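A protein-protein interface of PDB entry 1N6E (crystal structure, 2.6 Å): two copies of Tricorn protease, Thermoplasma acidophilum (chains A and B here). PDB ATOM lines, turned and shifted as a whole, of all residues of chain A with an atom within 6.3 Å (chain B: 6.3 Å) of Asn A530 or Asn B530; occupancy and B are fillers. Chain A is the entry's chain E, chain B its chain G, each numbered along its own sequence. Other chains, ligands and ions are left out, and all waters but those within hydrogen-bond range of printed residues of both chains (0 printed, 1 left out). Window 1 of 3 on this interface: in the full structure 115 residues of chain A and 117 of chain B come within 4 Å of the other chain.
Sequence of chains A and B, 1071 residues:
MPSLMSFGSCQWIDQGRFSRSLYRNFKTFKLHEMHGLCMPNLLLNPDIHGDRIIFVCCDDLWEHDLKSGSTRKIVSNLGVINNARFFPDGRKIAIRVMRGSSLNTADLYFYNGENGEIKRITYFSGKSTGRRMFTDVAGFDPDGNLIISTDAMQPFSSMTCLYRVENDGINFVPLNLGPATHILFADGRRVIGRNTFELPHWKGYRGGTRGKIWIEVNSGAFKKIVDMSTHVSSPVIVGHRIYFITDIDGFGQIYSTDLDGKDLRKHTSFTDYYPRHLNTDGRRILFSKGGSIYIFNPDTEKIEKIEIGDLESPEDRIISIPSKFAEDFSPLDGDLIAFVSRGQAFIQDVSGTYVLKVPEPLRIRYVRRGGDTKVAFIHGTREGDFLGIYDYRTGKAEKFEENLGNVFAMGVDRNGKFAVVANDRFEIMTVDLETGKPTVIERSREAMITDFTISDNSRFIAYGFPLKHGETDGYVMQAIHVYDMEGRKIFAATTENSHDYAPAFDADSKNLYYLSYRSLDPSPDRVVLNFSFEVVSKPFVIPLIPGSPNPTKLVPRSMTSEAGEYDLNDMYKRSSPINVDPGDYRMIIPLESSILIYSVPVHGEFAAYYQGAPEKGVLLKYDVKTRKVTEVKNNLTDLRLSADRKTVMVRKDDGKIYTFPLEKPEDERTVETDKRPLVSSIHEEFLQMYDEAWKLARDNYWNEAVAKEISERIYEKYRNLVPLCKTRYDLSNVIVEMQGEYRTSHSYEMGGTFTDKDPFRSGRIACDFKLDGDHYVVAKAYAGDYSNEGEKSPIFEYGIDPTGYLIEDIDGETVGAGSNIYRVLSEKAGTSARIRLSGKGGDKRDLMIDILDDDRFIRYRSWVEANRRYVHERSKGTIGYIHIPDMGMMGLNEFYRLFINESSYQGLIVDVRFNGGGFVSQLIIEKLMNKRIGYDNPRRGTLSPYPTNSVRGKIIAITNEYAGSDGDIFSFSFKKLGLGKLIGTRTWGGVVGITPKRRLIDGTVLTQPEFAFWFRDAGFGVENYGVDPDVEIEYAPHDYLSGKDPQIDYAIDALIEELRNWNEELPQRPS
The side-chain hydroxyl (OH) of Tyr A475 lies close to the side-chain amide oxygen (OD1) of Asn B949 (3.2 Å). The side-chain hydroxyl of Ser A532 lies within hydrogen-bond range of the side-chain hydroxyl of Ser B532, 3.1 Å away. The backbone NH (N) of Leu B529 is in hydrogen-bond range of the side-chain hydroxyl (OH) of Tyr A475. The backbone carbonyl oxygen (O) of Phe A531 lies close to the side-chain amide oxygen (OD1) of Asn B530 (3.2 Å). OD1 of Asp A525 sits at hydrogen-bond distance from N of Phe B533 (2.4 Å). The backbone NH of Arg A526 sits at hydrogen-bond distance from the backbone carbonyl oxygen of Phe B533 (2.8 Å). The side-chain carboxylate (OE1) of Glu A926 lies within salt-bridge range of the side-chain amino group (NZ) of Lys B927 (3.7 Å).
The side-chain hydroxyl (OG) of Ser B532 sits at hydrogen-bond distance from the side-chain carboxylate (OE1) of Glu B534, at 2.7 Å. N of Ser B523 is in hydrogen-bond range of O of Ser B532 (2.9 Å).
Val B528 touches Tyr A475. Ser B532 touches Asn A530 (CB to OD1, 3.6 Å). Ser A532 touches Asp B525 (CB to OD1, 2.8 Å). Ser A532 touches Asn B530 (CB to OD1, 3.6 Å). Phe B533 touches Tyr A896 (CE1 to CD1, 3.7 Å).
Of chain B, only Asn B530 (3.5 Å), Phe B531 (3.2 Å) and Ser B532 (3.6 Å) come within 4 Å of Asn A530. Of chain A, only Asn A530, Phe A531 and Ser A532 come within 4 Å of Asn B530. Printed residues of chain A within 4 Å of Glu B926: Glu A926 and Lys A927. Printed residues of chain B within 4 Å of Asn A949: Tyr B475 (2.2 Å). Printed residues of chain B within 4 Å of Leu A529: Tyr B475 and Leu B923. The nearest residue of chain B that does not touch Asn A530 is Leu B923 (4.7 Å). The nearest residue of chain A that does not touch Asn B530 is Leu A923 (4.5 Å).
Of the 16 printed residues of chain A, 16 touch a printed residue of chain B. Hydrophobic or aromatic side chains of chain A that line the printed part of chain B: Tyr A475, Val A528, Leu A529, Phe A531, Phe A533, Tyr A896 and Leu A923. Among the printed residues, 33 pairs touch across the chains. Among the printed residues, Asp or Glu carboxylates within 4 Å of a Lys or Arg side-chain nitrogen of the other chain: Glu A926 with Lys B927 and Lys A927 with Glu B926.
Asp A525 touches Phe B533, and with the chains exchanged Phe A533 touches Asp B525. Asn A530 touches Phe B531, and with the chains exchanged Phe A531 touches Asn B530. Glu B926 touches its own counterpart, Glu A926.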
ATOM      1  N   TYR A 475     -20.480   5.309   5.451  1.00  0.00           N
ATOM      2  CA  TYR A 475     -21.373   4.868   4.401  1.00  0.00           C
ATOM      3  C   TYR A 475     -22.127   6.039   3.791  1.00  0.00           C
ATOM      4  O   TYR A 475     -22.502   7.003   4.468  1.00  0.00           O
ATOM      5  CB  TYR A 475     -22.349   3.814   4.943  1.00  0.00           C
ATOM      6  CG  TYR A 475     -21.714   2.459   5.236  1.00  0.00           C
ATOM      7  CD1 TYR A 475     -21.132   2.176   6.506  1.00  0.00           C
ATOM      8  CD2 TYR A 475     -21.600   1.498   4.234  1.00  0.00           C
ATOM      9  CE1 TYR A 475     -20.438   0.956   6.749  1.00  0.00           C
ATOM     10  CE2 TYR A 475     -20.916   0.300   4.463  1.00  0.00           C
ATOM     11  CZ  TYR A 475     -20.336   0.027   5.708  1.00  0.00           C
ATOM     12  OH  TYR A 475     -19.663  -1.161   5.873  1.00  0.00           O
ATOM     13  N   SER A 523     -27.284 -13.985   4.058  1.00  0.00           N
ATOM     14  CA  SER A 523     -27.003 -15.257   3.394  1.00  0.00           C
ATOM     15  C   SER A 523     -25.739 -15.759   4.071  1.00  0.00           C
ATOM     16  O   SER A 523     -24.831 -14.987   4.339  1.00  0.00           O
ATOM     17  CB  SER A 523     -26.721 -15.092   1.905  1.00  0.00           C
ATOM     18  OG  SER A 523     -27.805 -14.519   1.220  1.00  0.00           O
ATOM     19  N   PRO A 524     -25.661 -17.062   4.357  1.00  0.00           N
ATOM     20  CA  PRO A 524     -24.494 -17.666   5.003  1.00  0.00           C
ATOM     21  C   PRO A 524     -23.316 -17.895   4.036  1.00  0.00           C
ATOM     22  O   PRO A 524     -23.497 -18.142   2.839  1.00  0.00           O
ATOM     23  CB  PRO A 524     -25.059 -18.979   5.516  1.00  0.00           C
ATOM     24  CG  PRO A 524     -25.997 -19.366   4.411  1.00  0.00           C
ATOM     25  CD  PRO A 524     -26.733 -18.063   4.174  1.00  0.00           C
ATOM     26  N   ASP A 525     -22.115 -17.814   4.594  1.00  0.00           N
ATOM     27  CA  ASP A 525     -20.860 -18.038   3.901  1.00  0.00           C
ATOM     28  C   ASP A 525     -20.623 -19.558   3.959  1.00  0.00           C
ATOM     29  O   ASP A 525     -20.796 -20.153   5.005  1.00  0.00           O
ATOM     30  CB  ASP A 525     -19.729 -17.320   4.663  1.00  0.00           C
ATOM     31  CG  ASP A 525     -18.424 -17.347   3.923  1.00  0.00           C
ATOM     32  OD1 ASP A 525     -18.070 -16.295   3.348  1.00  0.00           O
ATOM     33  OD2 ASP A 525     -17.765 -18.413   3.917  1.00  0.00           O
ATOM     34  N   ARG A 526     -20.192 -20.174   2.869  1.00  0.00           N
ATOM     35  CA  ARG A 526     -19.973 -21.598   2.899  1.00  0.00           C
ATOM     36  C   ARG A 526     -18.653 -22.094   3.513  1.00  0.00           C
ATOM     37  O   ARG A 526     -18.498 -23.280   3.786  1.00  0.00           O
ATOM     38  CB  ARG A 526     -20.094 -22.182   1.498  1.00  0.00           C
ATOM     39  CG  ARG A 526     -21.456 -21.947   0.813  1.00  0.00           C
ATOM     40  CD  ARG A 526     -22.604 -22.300   1.733  1.00  0.00           C
ATOM     41  NE  ARG A 526     -23.910 -21.928   1.174  1.00  0.00           N
ATOM     42  CZ  ARG A 526     -25.074 -22.093   1.807  1.00  0.00           C
ATOM     43  NH1 ARG A 526     -26.222 -21.736   1.244  1.00  0.00           N
ATOM     44  NH2 ARG A 526     -25.088 -22.614   3.022  1.00  0.00           N
ATOM     45  N   VAL A 528     -16.368 -19.711   5.771  1.00  0.00           N
ATOM     46  CA  VAL A 528     -16.042 -18.975   6.984  1.00  0.00           C
ATOM     47  C   VAL A 528     -17.280 -18.634   7.763  1.00  0.00           C
ATOM     48  O   VAL A 528     -18.318 -18.469   7.173  1.00  0.00           O
ATOM     49  CB  VAL A 528     -15.305 -17.638   6.601  1.00  0.00           C
ATOM     50  CG1 VAL A 528     -15.016 -16.798   7.870  1.00  0.00           C
ATOM     51  CG2 VAL A 528     -13.991 -17.974   5.832  1.00  0.00           C
ATOM     52  N   LEU A 529     -17.176 -18.525   9.075  1.00  0.00           N
ATOM     53  CA  LEU A 529     -18.337 -18.144   9.865  1.00  0.00           C
ATOM     54  C   LEU A 529     -18.610 -16.679   9.504  1.00  0.00           C
ATOM     55  O   LEU A 529     -17.991 -15.768  10.059  1.00  0.00           O
ATOM     56  CB  LEU A 529     -18.048 -18.268  11.358  1.00  0.00           C
ATOM     57  CG  LEU A 529     -19.108 -17.549  12.181  1.00  0.00           C
ATOM     58  CD1 LEU A 529     -20.451 -18.223  11.916  1.00  0.00           C
ATOM     59  CD2 LEU A 529     -18.760 -17.541  13.672  1.00  0.00           C
ATOM     60  N   ASN A 530     -19.517 -16.452   8.562  1.00  0.00           N
ATOM     61  CA  ASN A 530     -19.808 -15.105   8.116  1.00  0.00           C
ATOM     62  C   ASN A 530     -21.153 -15.017   7.407  1.00  0.00           C
ATOM     63  O   ASN A 530     -21.717 -16.034   7.051  1.00  0.00           O
ATOM     64  CB  ASN A 530     -18.711 -14.652   7.171  1.00  0.00           C
ATOM     65  CG  ASN A 530     -18.905 -13.214   6.700  1.00  0.00           C
ATOM     66  OD1 ASN A 530     -18.551 -12.892   5.561  1.00  0.00           O
ATOM     67  ND2 ASN A 530     -19.441 -12.334   7.571  1.00  0.00           N
ATOM     68  N   PHE A 531     -21.674 -13.810   7.228  1.00  0.00           N
ATOM     69  CA  PHE A 531     -22.953 -13.612   6.559  1.00  0.00           C
ATOM     70  C   PHE A 531     -22.918 -12.303   5.815  1.00  0.00           C
ATOM     71  O   PHE A 531     -22.257 -11.376   6.245  1.00  0.00           O
ATOM     72  CB  PHE A 531     -24.126 -13.556   7.563  1.00  0.00           C
ATOM     73  CG  PHE A 531     -24.393 -14.847   8.282  1.00  0.00           C
ATOM     74  CD1 PHE A 531     -23.674 -15.182   9.415  1.00  0.00           C
ATOM     75  CD2 PHE A 531     -25.276 -15.782   7.759  1.00  0.00           C
ATOM     76  CE1 PHE A 531     -23.831 -16.421  10.031  1.00  0.00           C
ATOM     77  CE2 PHE A 531     -25.434 -17.040   8.380  1.00  0.00           C
ATOM     78  CZ  PHE A 531     -24.694 -17.346   9.508  1.00  0.00           C
ATOM     79  N   SER A 532     -23.626 -12.205   4.703  1.00  0.00           N
ATOM     80  CA  SER A 532     -23.630 -10.937   3.997  1.00  0.00           C
ATOM     81  C   SER A 532     -24.957 -10.739   3.304  1.00  0.00           C
ATOM     82  O   SER A 532     -25.721 -11.682   3.190  1.00  0.00           O
ATOM     83  CB  SER A 532     -22.477 -10.880   2.975  1.00  0.00           C
ATOM     84  OG  SER A 532     -22.717 -11.743   1.878  1.00  0.00           O
ATOM     85  N   PHE A 533     -25.239  -9.515   2.864  1.00  0.00           N
ATOM     86  CA  PHE A 533     -26.467  -9.236   2.145  1.00  0.00           C
ATOM     87  C   PHE A 533     -26.284  -9.391   0.637  1.00  0.00           C
ATOM     88  O   PHE A 533     -25.735  -8.529  -0.047  1.00  0.00           O
ATOM     89  CB  PHE A 533     -26.951  -7.855   2.518  1.00  0.00           C
ATOM     90  CG  PHE A 533     -27.093  -7.681   3.995  1.00  0.00           C
ATOM     91  CD1 PHE A 533     -26.097  -7.048   4.734  1.00  0.00           C
ATOM     92  CD2 PHE A 533     -28.218  -8.201   4.664  1.00  0.00           C
ATOM     93  CE1 PHE A 533     -26.207  -6.929   6.138  1.00  0.00           C
ATOM     94  CE2 PHE A 533     -28.351  -8.099   6.061  1.00  0.00           C
ATOM     95  CZ  PHE A 533     -27.340  -7.453   6.801  1.00  0.00           C
ATOM     96  N   TYR A 896      -8.202 -16.462   3.705  1.00  0.00           N
ATOM     97  CA  TYR A 896      -9.045 -17.462   4.323  1.00  0.00           C
ATOM     98  C   TYR A 896      -8.585 -18.877   4.005  1.00  0.00           C
ATOM     99  O   TYR A 896      -8.599 -19.739   4.901  1.00  0.00           O
ATOM    100  CB  TYR A 896     -10.518 -17.256   3.950  1.00  0.00           C
ATOM    101  CG  TYR A 896     -11.113 -16.024   4.619  1.00  0.00           C
ATOM    102  CD1 TYR A 896     -11.404 -14.889   3.865  1.00  0.00           C
ATOM    103  CD2 TYR A 896     -11.323 -15.985   6.003  1.00  0.00           C
ATOM    104  CE1 TYR A 896     -11.893 -13.751   4.462  1.00  0.00           C
ATOM    105  CE2 TYR A 896     -11.791 -14.854   6.611  1.00  0.00           C
ATOM    106  CZ  TYR A 896     -12.084 -13.733   5.836  1.00  0.00           C
ATOM    107  OH  TYR A 896     -12.588 -12.569   6.382  1.00  0.00           O
ATOM    108  N   LEU A 923     -10.563  -5.428   6.258  1.00  0.00           N
ATOM    109  CA  LEU A 923     -11.353  -6.646   6.521  1.00  0.00           C
ATOM    110  C   LEU A 923     -10.476  -7.758   7.079  1.00  0.00           C
ATOM    111  O   LEU A 923     -10.944  -8.593   7.876  1.00  0.00           O
ATOM    112  CB  LEU A 923     -12.069  -7.157   5.253  1.00  0.00           C
ATOM    113  CG  LEU A 923     -12.871  -6.074   4.506  1.00  0.00           C
ATOM    114  CD1 LEU A 923     -13.529  -6.604   3.224  1.00  0.00           C
ATOM    115  CD2 LEU A 923     -13.885  -5.512   5.461  1.00  0.00           C
ATOM    116  N   GLU A 926      -9.318  -6.888  10.776  1.00  0.00           N
ATOM    117  CA  GLU A 926     -10.485  -7.153  11.666  1.00  0.00           C
ATOM    118  C   GLU A 926     -10.489  -8.586  12.210  1.00  0.00           C
ATOM    119  O   GLU A 926     -10.738  -8.824  13.405  1.00  0.00           O
ATOM    120  CB  GLU A 926     -11.800  -6.879  10.908  1.00  0.00           C
ATOM    121  CG  GLU A 926     -13.058  -7.035  11.727  1.00  0.00           C
ATOM    122  CD  GLU A 926     -14.331  -6.684  10.920  1.00  0.00           C
ATOM    123  OE1 GLU A 926     -14.513  -7.249   9.803  1.00  0.00           O
ATOM    124  OE2 GLU A 926     -15.155  -5.841  11.397  1.00  0.00           O
ATOM    125  N   LYS A 927     -10.193  -9.529  11.321  1.00  0.00           N
ATOM    126  CA  LYS A 927     -10.108 -10.928  11.696  1.00  0.00           C
ATOM    127  C   LYS A 927      -8.933 -11.117  12.669  1.00  0.00           C
ATOM    128  O   LYS A 927      -9.104 -11.715  13.735  1.00  0.00           O
ATOM    129  CB  LYS A 927      -9.884 -11.777  10.462  1.00  0.00           C
ATOM    130  CG  LYS A 927     -10.993 -12.727  10.212  1.00  0.00           C
ATOM    131  CD  LYS A 927     -12.222 -11.952   9.863  1.00  0.00           C
ATOM    132  CE  LYS A 927     -13.400 -12.859   9.627  1.00  0.00           C
ATOM    133  NZ  LYS A 927     -14.499 -11.988   9.117  1.00  0.00           N
ATOM    134  N   ASN A 949     -13.376 -16.810  14.662  1.00  0.00           N
ATOM    135  CA  ASN A 949     -12.376 -16.249  13.811  1.00  0.00           C
ATOM    136  C   ASN A 949     -11.327 -15.499  14.560  1.00  0.00           C
ATOM    137  O   ASN A 949     -11.014 -14.344  14.255  1.00  0.00           O
ATOM    138  CB  ASN A 949     -13.017 -15.348  12.774  1.00  0.00           C
ATOM    139  CG  ASN A 949     -13.778 -16.132  11.758  1.00  0.00           C
ATOM    140  OD1 ASN A 949     -14.877 -15.735  11.355  1.00  0.00           O
ATOM    141  ND2 ASN A 949     -13.215 -17.277  11.338  1.00  0.00           N
ATOM    142  N   TYR B 475     -12.265 -24.175  13.190  1.00  0.00           N
ATOM    143  CA  TYR B 475     -12.937 -24.765  12.073  1.00  0.00           C
ATOM    144  C   TYR B 475     -12.656 -26.285  12.004  1.00  0.00           C
ATOM    145  O   TYR B 475     -11.559 -26.776  12.340  1.00  0.00           O
ATOM    146  CB  TYR B 475     -12.513 -24.057  10.781  1.00  0.00           C
ATOM    147  CG  TYR B 475     -13.035 -22.643  10.653  1.00  0.00           C
ATOM    148  CD1 TYR B 475     -12.303 -21.550  11.114  1.00  0.00           C
ATOM    149  CD2 TYR B 475     -14.295 -22.408  10.125  1.00  0.00           C
ATOM    150  CE1 TYR B 475     -12.819 -20.259  11.056  1.00  0.00           C
ATOM    151  CE2 TYR B 475     -14.837 -21.126  10.065  1.00  0.00           C
ATOM    152  CZ  TYR B 475     -14.098 -20.051  10.536  1.00  0.00           C
ATOM    153  OH  TYR B 475     -14.667 -18.788  10.526  1.00  0.00           O
ATOM    154  N   SER B 523     -17.881 -13.012  -3.010  1.00  0.00           N
ATOM    155  CA  SER B 523     -19.037 -12.301  -3.550  1.00  0.00           C
ATOM    156  C   SER B 523     -19.225 -11.102  -2.655  1.00  0.00           C
ATOM    157  O   SER B 523     -19.169 -11.219  -1.441  1.00  0.00           O
ATOM    158  CB  SER B 523     -20.320 -13.137  -3.516  1.00  0.00           C
ATOM    159  OG  SER B 523     -20.173 -14.328  -4.248  1.00  0.00           O
ATOM    160  N   PRO B 524     -19.463  -9.925  -3.248  1.00  0.00           N
ATOM    161  CA  PRO B 524     -19.675  -8.667  -2.500  1.00  0.00           C
ATOM    162  C   PRO B 524     -21.048  -8.559  -1.831  1.00  0.00           C
ATOM    163  O   PRO B 524     -22.023  -9.041  -2.353  1.00  0.00           O
ATOM    164  CB  PRO B 524     -19.529  -7.606  -3.577  1.00  0.00           C
ATOM    165  CG  PRO B 524     -20.220  -8.294  -4.755  1.00  0.00           C
ATOM    166  CD  PRO B 524     -19.591  -9.693  -4.703  1.00  0.00           C
ATOM    167  N   ASP B 525     -21.067  -7.904  -0.678  1.00  0.00           N
ATOM    168  CA  ASP B 525     -22.243  -7.619   0.125  1.00  0.00           C
ATOM    169  C   ASP B 525     -22.851  -6.350  -0.500  1.00  0.00           C
ATOM    170  O   ASP B 525     -22.130  -5.426  -0.872  1.00  0.00           O
ATOM    171  CB  ASP B 525     -21.813  -7.322   1.563  1.00  0.00           C
ATOM    172  CG  ASP B 525     -22.976  -7.240   2.533  1.00  0.00           C
ATOM    173  OD1 ASP B 525     -23.126  -8.179   3.331  1.00  0.00           O
ATOM    174  OD2 ASP B 525     -23.712  -6.234   2.504  1.00  0.00           O
ATOM    175  N   ARG B 526     -24.171  -6.278  -0.619  1.00  0.00           N
ATOM    176  CA  ARG B 526     -24.765  -5.102  -1.261  1.00  0.00           C
ATOM    177  C   ARG B 526     -25.016  -3.920  -0.321  1.00  0.00           C
ATOM    178  O   ARG B 526     -25.357  -2.825  -0.778  1.00  0.00           O
ATOM    179  CB  ARG B 526     -26.094  -5.504  -1.936  1.00  0.00           C
ATOM    180  CG  ARG B 526     -25.948  -6.630  -2.940  1.00  0.00           C
ATOM    181  CD  ARG B 526     -24.865  -6.304  -3.949  1.00  0.00           C
ATOM    182  NE  ARG B 526     -24.670  -7.349  -4.952  1.00  0.00           N
ATOM    183  CZ  ARG B 526     -23.758  -7.287  -5.927  1.00  0.00           C
ATOM    184  NH1 ARG B 526     -23.638  -8.269  -6.830  1.00  0.00           N
ATOM    185  NH2 ARG B 526     -22.948  -6.238  -5.997  1.00  0.00           N
ATOM    186  N   VAL B 528     -23.145  -3.636   3.255  1.00  0.00           N
ATOM    187  CA  VAL B 528     -22.013  -3.416   4.130  1.00  0.00           C
ATOM    188  C   VAL B 528     -20.736  -3.732   3.401  1.00  0.00           C
ATOM    189  O   VAL B 528     -20.758  -4.564   2.511  1.00  0.00           O
ATOM    190  CB  VAL B 528     -22.119  -4.345   5.342  1.00  0.00           C
ATOM    191  CG1 VAL B 528     -20.930  -4.145   6.234  1.00  0.00           C
ATOM    192  CG2 VAL B 528     -23.420  -4.078   6.091  1.00  0.00           C
ATOM    193  N   LEU B 529     -19.631  -3.081   3.779  1.00  0.00           N
ATOM    194  CA  LEU B 529     -18.351  -3.374   3.136  1.00  0.00           C
ATOM    195  C   LEU B 529     -17.964  -4.774   3.609  1.00  0.00           C
ATOM    196  O   LEU B 529     -17.383  -4.943   4.672  1.00  0.00           O
ATOM    197  CB  LEU B 529     -17.305  -2.377   3.577  1.00  0.00           C
ATOM    198  CG  LEU B 529     -15.904  -2.885   3.154  1.00  0.00           C
ATOM    199  CD1 LEU B 529     -15.868  -3.030   1.639  1.00  0.00           C
ATOM    200  CD2 LEU B 529     -14.797  -1.957   3.643  1.00  0.00           C
ATOM    201  N   ASN B 530     -18.318  -5.788   2.843  1.00  0.00           N
ATOM    202  CA  ASN B 530     -18.040  -7.150   3.257  1.00  0.00           C
ATOM    203  C   ASN B 530     -18.061  -8.088   2.036  1.00  0.00           C
ATOM    204  O   ASN B 530     -18.494  -7.682   0.932  1.00  0.00           O
ATOM    205  CB  ASN B 530     -19.097  -7.561   4.264  1.00  0.00           C
ATOM    206  CG  ASN B 530     -18.879  -8.954   4.796  1.00  0.00           C
ATOM    207  OD1 ASN B 530     -19.841  -9.648   5.173  1.00  0.00           O
ATOM    208  ND2 ASN B 530     -17.624  -9.383   4.841  1.00  0.00           N
ATOM    209  N   PHE B 531     -17.589  -9.323   2.226  1.00  0.00           N
ATOM    210  CA  PHE B 531     -17.539 -10.317   1.157  1.00  0.00           C
ATOM    211  C   PHE B 531     -17.658 -11.674   1.760  1.00  0.00           C
ATOM    212  O   PHE B 531     -17.190 -11.888   2.876  1.00  0.00           O
ATOM    213  CB  PHE B 531     -16.213 -10.266   0.411  1.00  0.00           C
ATOM    214  CG  PHE B 531     -16.005  -9.000  -0.356  1.00  0.00           C
ATOM    215  CD1 PHE B 531     -15.450  -7.881   0.269  1.00  0.00           C
ATOM    216  CD2 PHE B 531     -16.422  -8.909  -1.695  1.00  0.00           C
ATOM    217  CE1 PHE B 531     -15.322  -6.675  -0.424  1.00  0.00           C
ATOM    218  CE2 PHE B 531     -16.294  -7.700  -2.403  1.00  0.00           C
ATOM    219  CZ  PHE B 531     -15.744  -6.572  -1.768  1.00  0.00           C
ATOM    220  N   SER B 532     -18.280 -12.611   1.057  1.00  0.00           N
ATOM    221  CA  SER B 532     -18.356 -13.956   1.620  1.00  0.00           C
ATOM    222  C   SER B 532     -18.274 -15.003   0.537  1.00  0.00           C
ATOM    223  O   SER B 532     -18.349 -14.670  -0.638  1.00  0.00           O
ATOM    224  CB  SER B 532     -19.638 -14.141   2.412  1.00  0.00           C
ATOM    225  OG  SER B 532     -20.723 -14.147   1.528  1.00  0.00           O
ATOM    226  N   PHE B 533     -18.089 -16.260   0.919  1.00  0.00           N
ATOM    227  CA  PHE B 533     -18.021 -17.303  -0.077  1.00  0.00           C
ATOM    228  C   PHE B 533     -19.389 -17.926  -0.278  1.00  0.00           C
ATOM    229  O   PHE B 533     -19.834 -18.745   0.518  1.00  0.00           O
ATOM    230  CB  PHE B 533     -16.978 -18.328   0.326  1.00  0.00           C
ATOM    231  CG  PHE B 533     -15.632 -17.729   0.536  1.00  0.00           C
ATOM    232  CD1 PHE B 533     -15.150 -17.494   1.822  1.00  0.00           C
ATOM    233  CD2 PHE B 533     -14.861 -17.327  -0.548  1.00  0.00           C
ATOM    234  CE1 PHE B 533     -13.908 -16.864   2.027  1.00  0.00           C
ATOM    235  CE2 PHE B 533     -13.629 -16.700  -0.346  1.00  0.00           C
ATOM    236  CZ  PHE B 533     -13.159 -16.467   0.957  1.00  0.00           C
ATOM    237  N   GLU B 534     -20.055 -17.498  -1.344  1.00  0.00           N
ATOM    238  CA  GLU B 534     -21.399 -17.978  -1.671  1.00  0.00           C
ATOM    239  C   GLU B 534     -21.383 -19.092  -2.726  1.00  0.00           C
ATOM    240  O   GLU B 534     -22.068 -20.097  -2.572  1.00  0.00           O
ATOM    241  CB  GLU B 534     -22.255 -16.836  -2.231  1.00  0.00           C
ATOM    242  CG  GLU B 534     -22.265 -15.560  -1.415  1.00  0.00           C
ATOM    243  CD  GLU B 534     -22.812 -15.800  -0.017  1.00  0.00           C
ATOM    244  OE1 GLU B 534     -22.097 -16.404   0.822  1.00  0.00           O
ATOM    245  OE2 GLU B 534     -23.962 -15.394   0.267  1.00  0.00           O
ATOM    246  N   TYR B 896     -27.088  -4.072  11.358  1.00  0.00           N
ATOM    247  CA  TYR B 896     -26.600  -3.321  10.215  1.00  0.00           C
ATOM    248  C   TYR B 896     -27.574  -2.236   9.719  1.00  0.00           C
ATOM    249  O   TYR B 896     -27.154  -1.154   9.297  1.00  0.00           O
ATOM    250  CB  TYR B 896     -26.217  -4.250   9.090  1.00  0.00           C
ATOM    251  CG  TYR B 896     -24.944  -5.029   9.402  1.00  0.00           C
ATOM    252  CD1 TYR B 896     -24.984  -6.420   9.558  1.00  0.00           C
ATOM    253  CD2 TYR B 896     -23.709  -4.365   9.606  1.00  0.00           C
ATOM    254  CE1 TYR B 896     -23.854  -7.132   9.909  1.00  0.00           C
ATOM    255  CE2 TYR B 896     -22.560  -5.071   9.961  1.00  0.00           C
ATOM    256  CZ  TYR B 896     -22.631  -6.461  10.114  1.00  0.00           C
ATOM    257  OH  TYR B 896     -21.503  -7.198  10.479  1.00  0.00           O
ATOM    258  N   LEU B 923     -19.769 -11.926  15.743  1.00  0.00           N
ATOM    259  CA  LEU B 923     -19.670 -11.176  14.497  1.00  0.00           C
ATOM    260  C   LEU B 923     -19.976  -9.694  14.704  1.00  0.00           C
ATOM    261  O   LEU B 923     -19.418  -8.836  14.011  1.00  0.00           O
ATOM    262  CB  LEU B 923     -20.632 -11.753  13.476  1.00  0.00           C
ATOM    263  CG  LEU B 923     -20.558 -13.280  13.287  1.00  0.00           C
ATOM    264  CD1 LEU B 923     -21.568 -13.793  12.217  1.00  0.00           C
ATOM    265  CD2 LEU B 923     -19.115 -13.624  12.890  1.00  0.00           C
ATOM    266  N   GLU B 926     -17.103  -7.881  16.764  1.00  0.00           N
ATOM    267  CA  GLU B 926     -15.983  -7.667  15.873  1.00  0.00           C
ATOM    268  C   GLU B 926     -16.093  -6.335  15.204  1.00  0.00           C
ATOM    269  O   GLU B 926     -15.099  -5.629  15.049  1.00  0.00           O
ATOM    270  CB  GLU B 926     -15.932  -8.794  14.829  1.00  0.00           C
ATOM    271  CG  GLU B 926     -14.805  -8.727  13.836  1.00  0.00           C
ATOM    272  CD  GLU B 926     -14.839  -9.884  12.819  1.00  0.00           C
ATOM    273  OE1 GLU B 926     -15.901 -10.103  12.193  1.00  0.00           O
ATOM    274  OE2 GLU B 926     -13.803 -10.575  12.630  1.00  0.00           O
ATOM    275  N   LYS B 927     -17.311  -5.978  14.808  1.00  0.00           N
ATOM    276  CA  LYS B 927     -17.553  -4.693  14.151  1.00  0.00           C
ATOM    277  C   LYS B 927     -17.305  -3.592  15.168  1.00  0.00           C
ATOM    278  O   LYS B 927     -16.569  -2.651  14.888  1.00  0.00           O
ATOM    279  CB  LYS B 927     -19.001  -4.611  13.659  1.00  0.00           C
ATOM    280  CG  LYS B 927     -19.125  -4.488  12.184  1.00  0.00           C
ATOM    281  CD  LYS B 927     -18.598  -5.727  11.542  1.00  0.00           C
ATOM    282  CE  LYS B 927     -18.639  -5.614  10.059  1.00  0.00           C
ATOM    283  NZ  LYS B 927     -18.158  -6.932   9.570  1.00  0.00           N
ATOM    284  N   ASN B 949     -15.968   0.060   8.703  1.00  0.00           N
ATOM    285  CA  ASN B 949     -16.841  -0.422   9.725  1.00  0.00           C
ATOM    286  C   ASN B 949     -16.383  -0.152  11.125  1.00  0.00           C
ATOM    287  O   ASN B 949     -16.347  -1.035  11.962  1.00  0.00           O
ATOM    288  CB  ASN B 949     -17.127  -1.900   9.520  1.00  0.00           C
ATOM    289  CG  ASN B 949     -17.989  -2.133   8.316  1.00  0.00           C
ATOM    290  OD1 ASN B 949     -17.775  -3.086   7.568  1.00  0.00           O
ATOM    291  ND2 ASN B 949     -18.952  -1.248   8.096  1.00  0.00           N
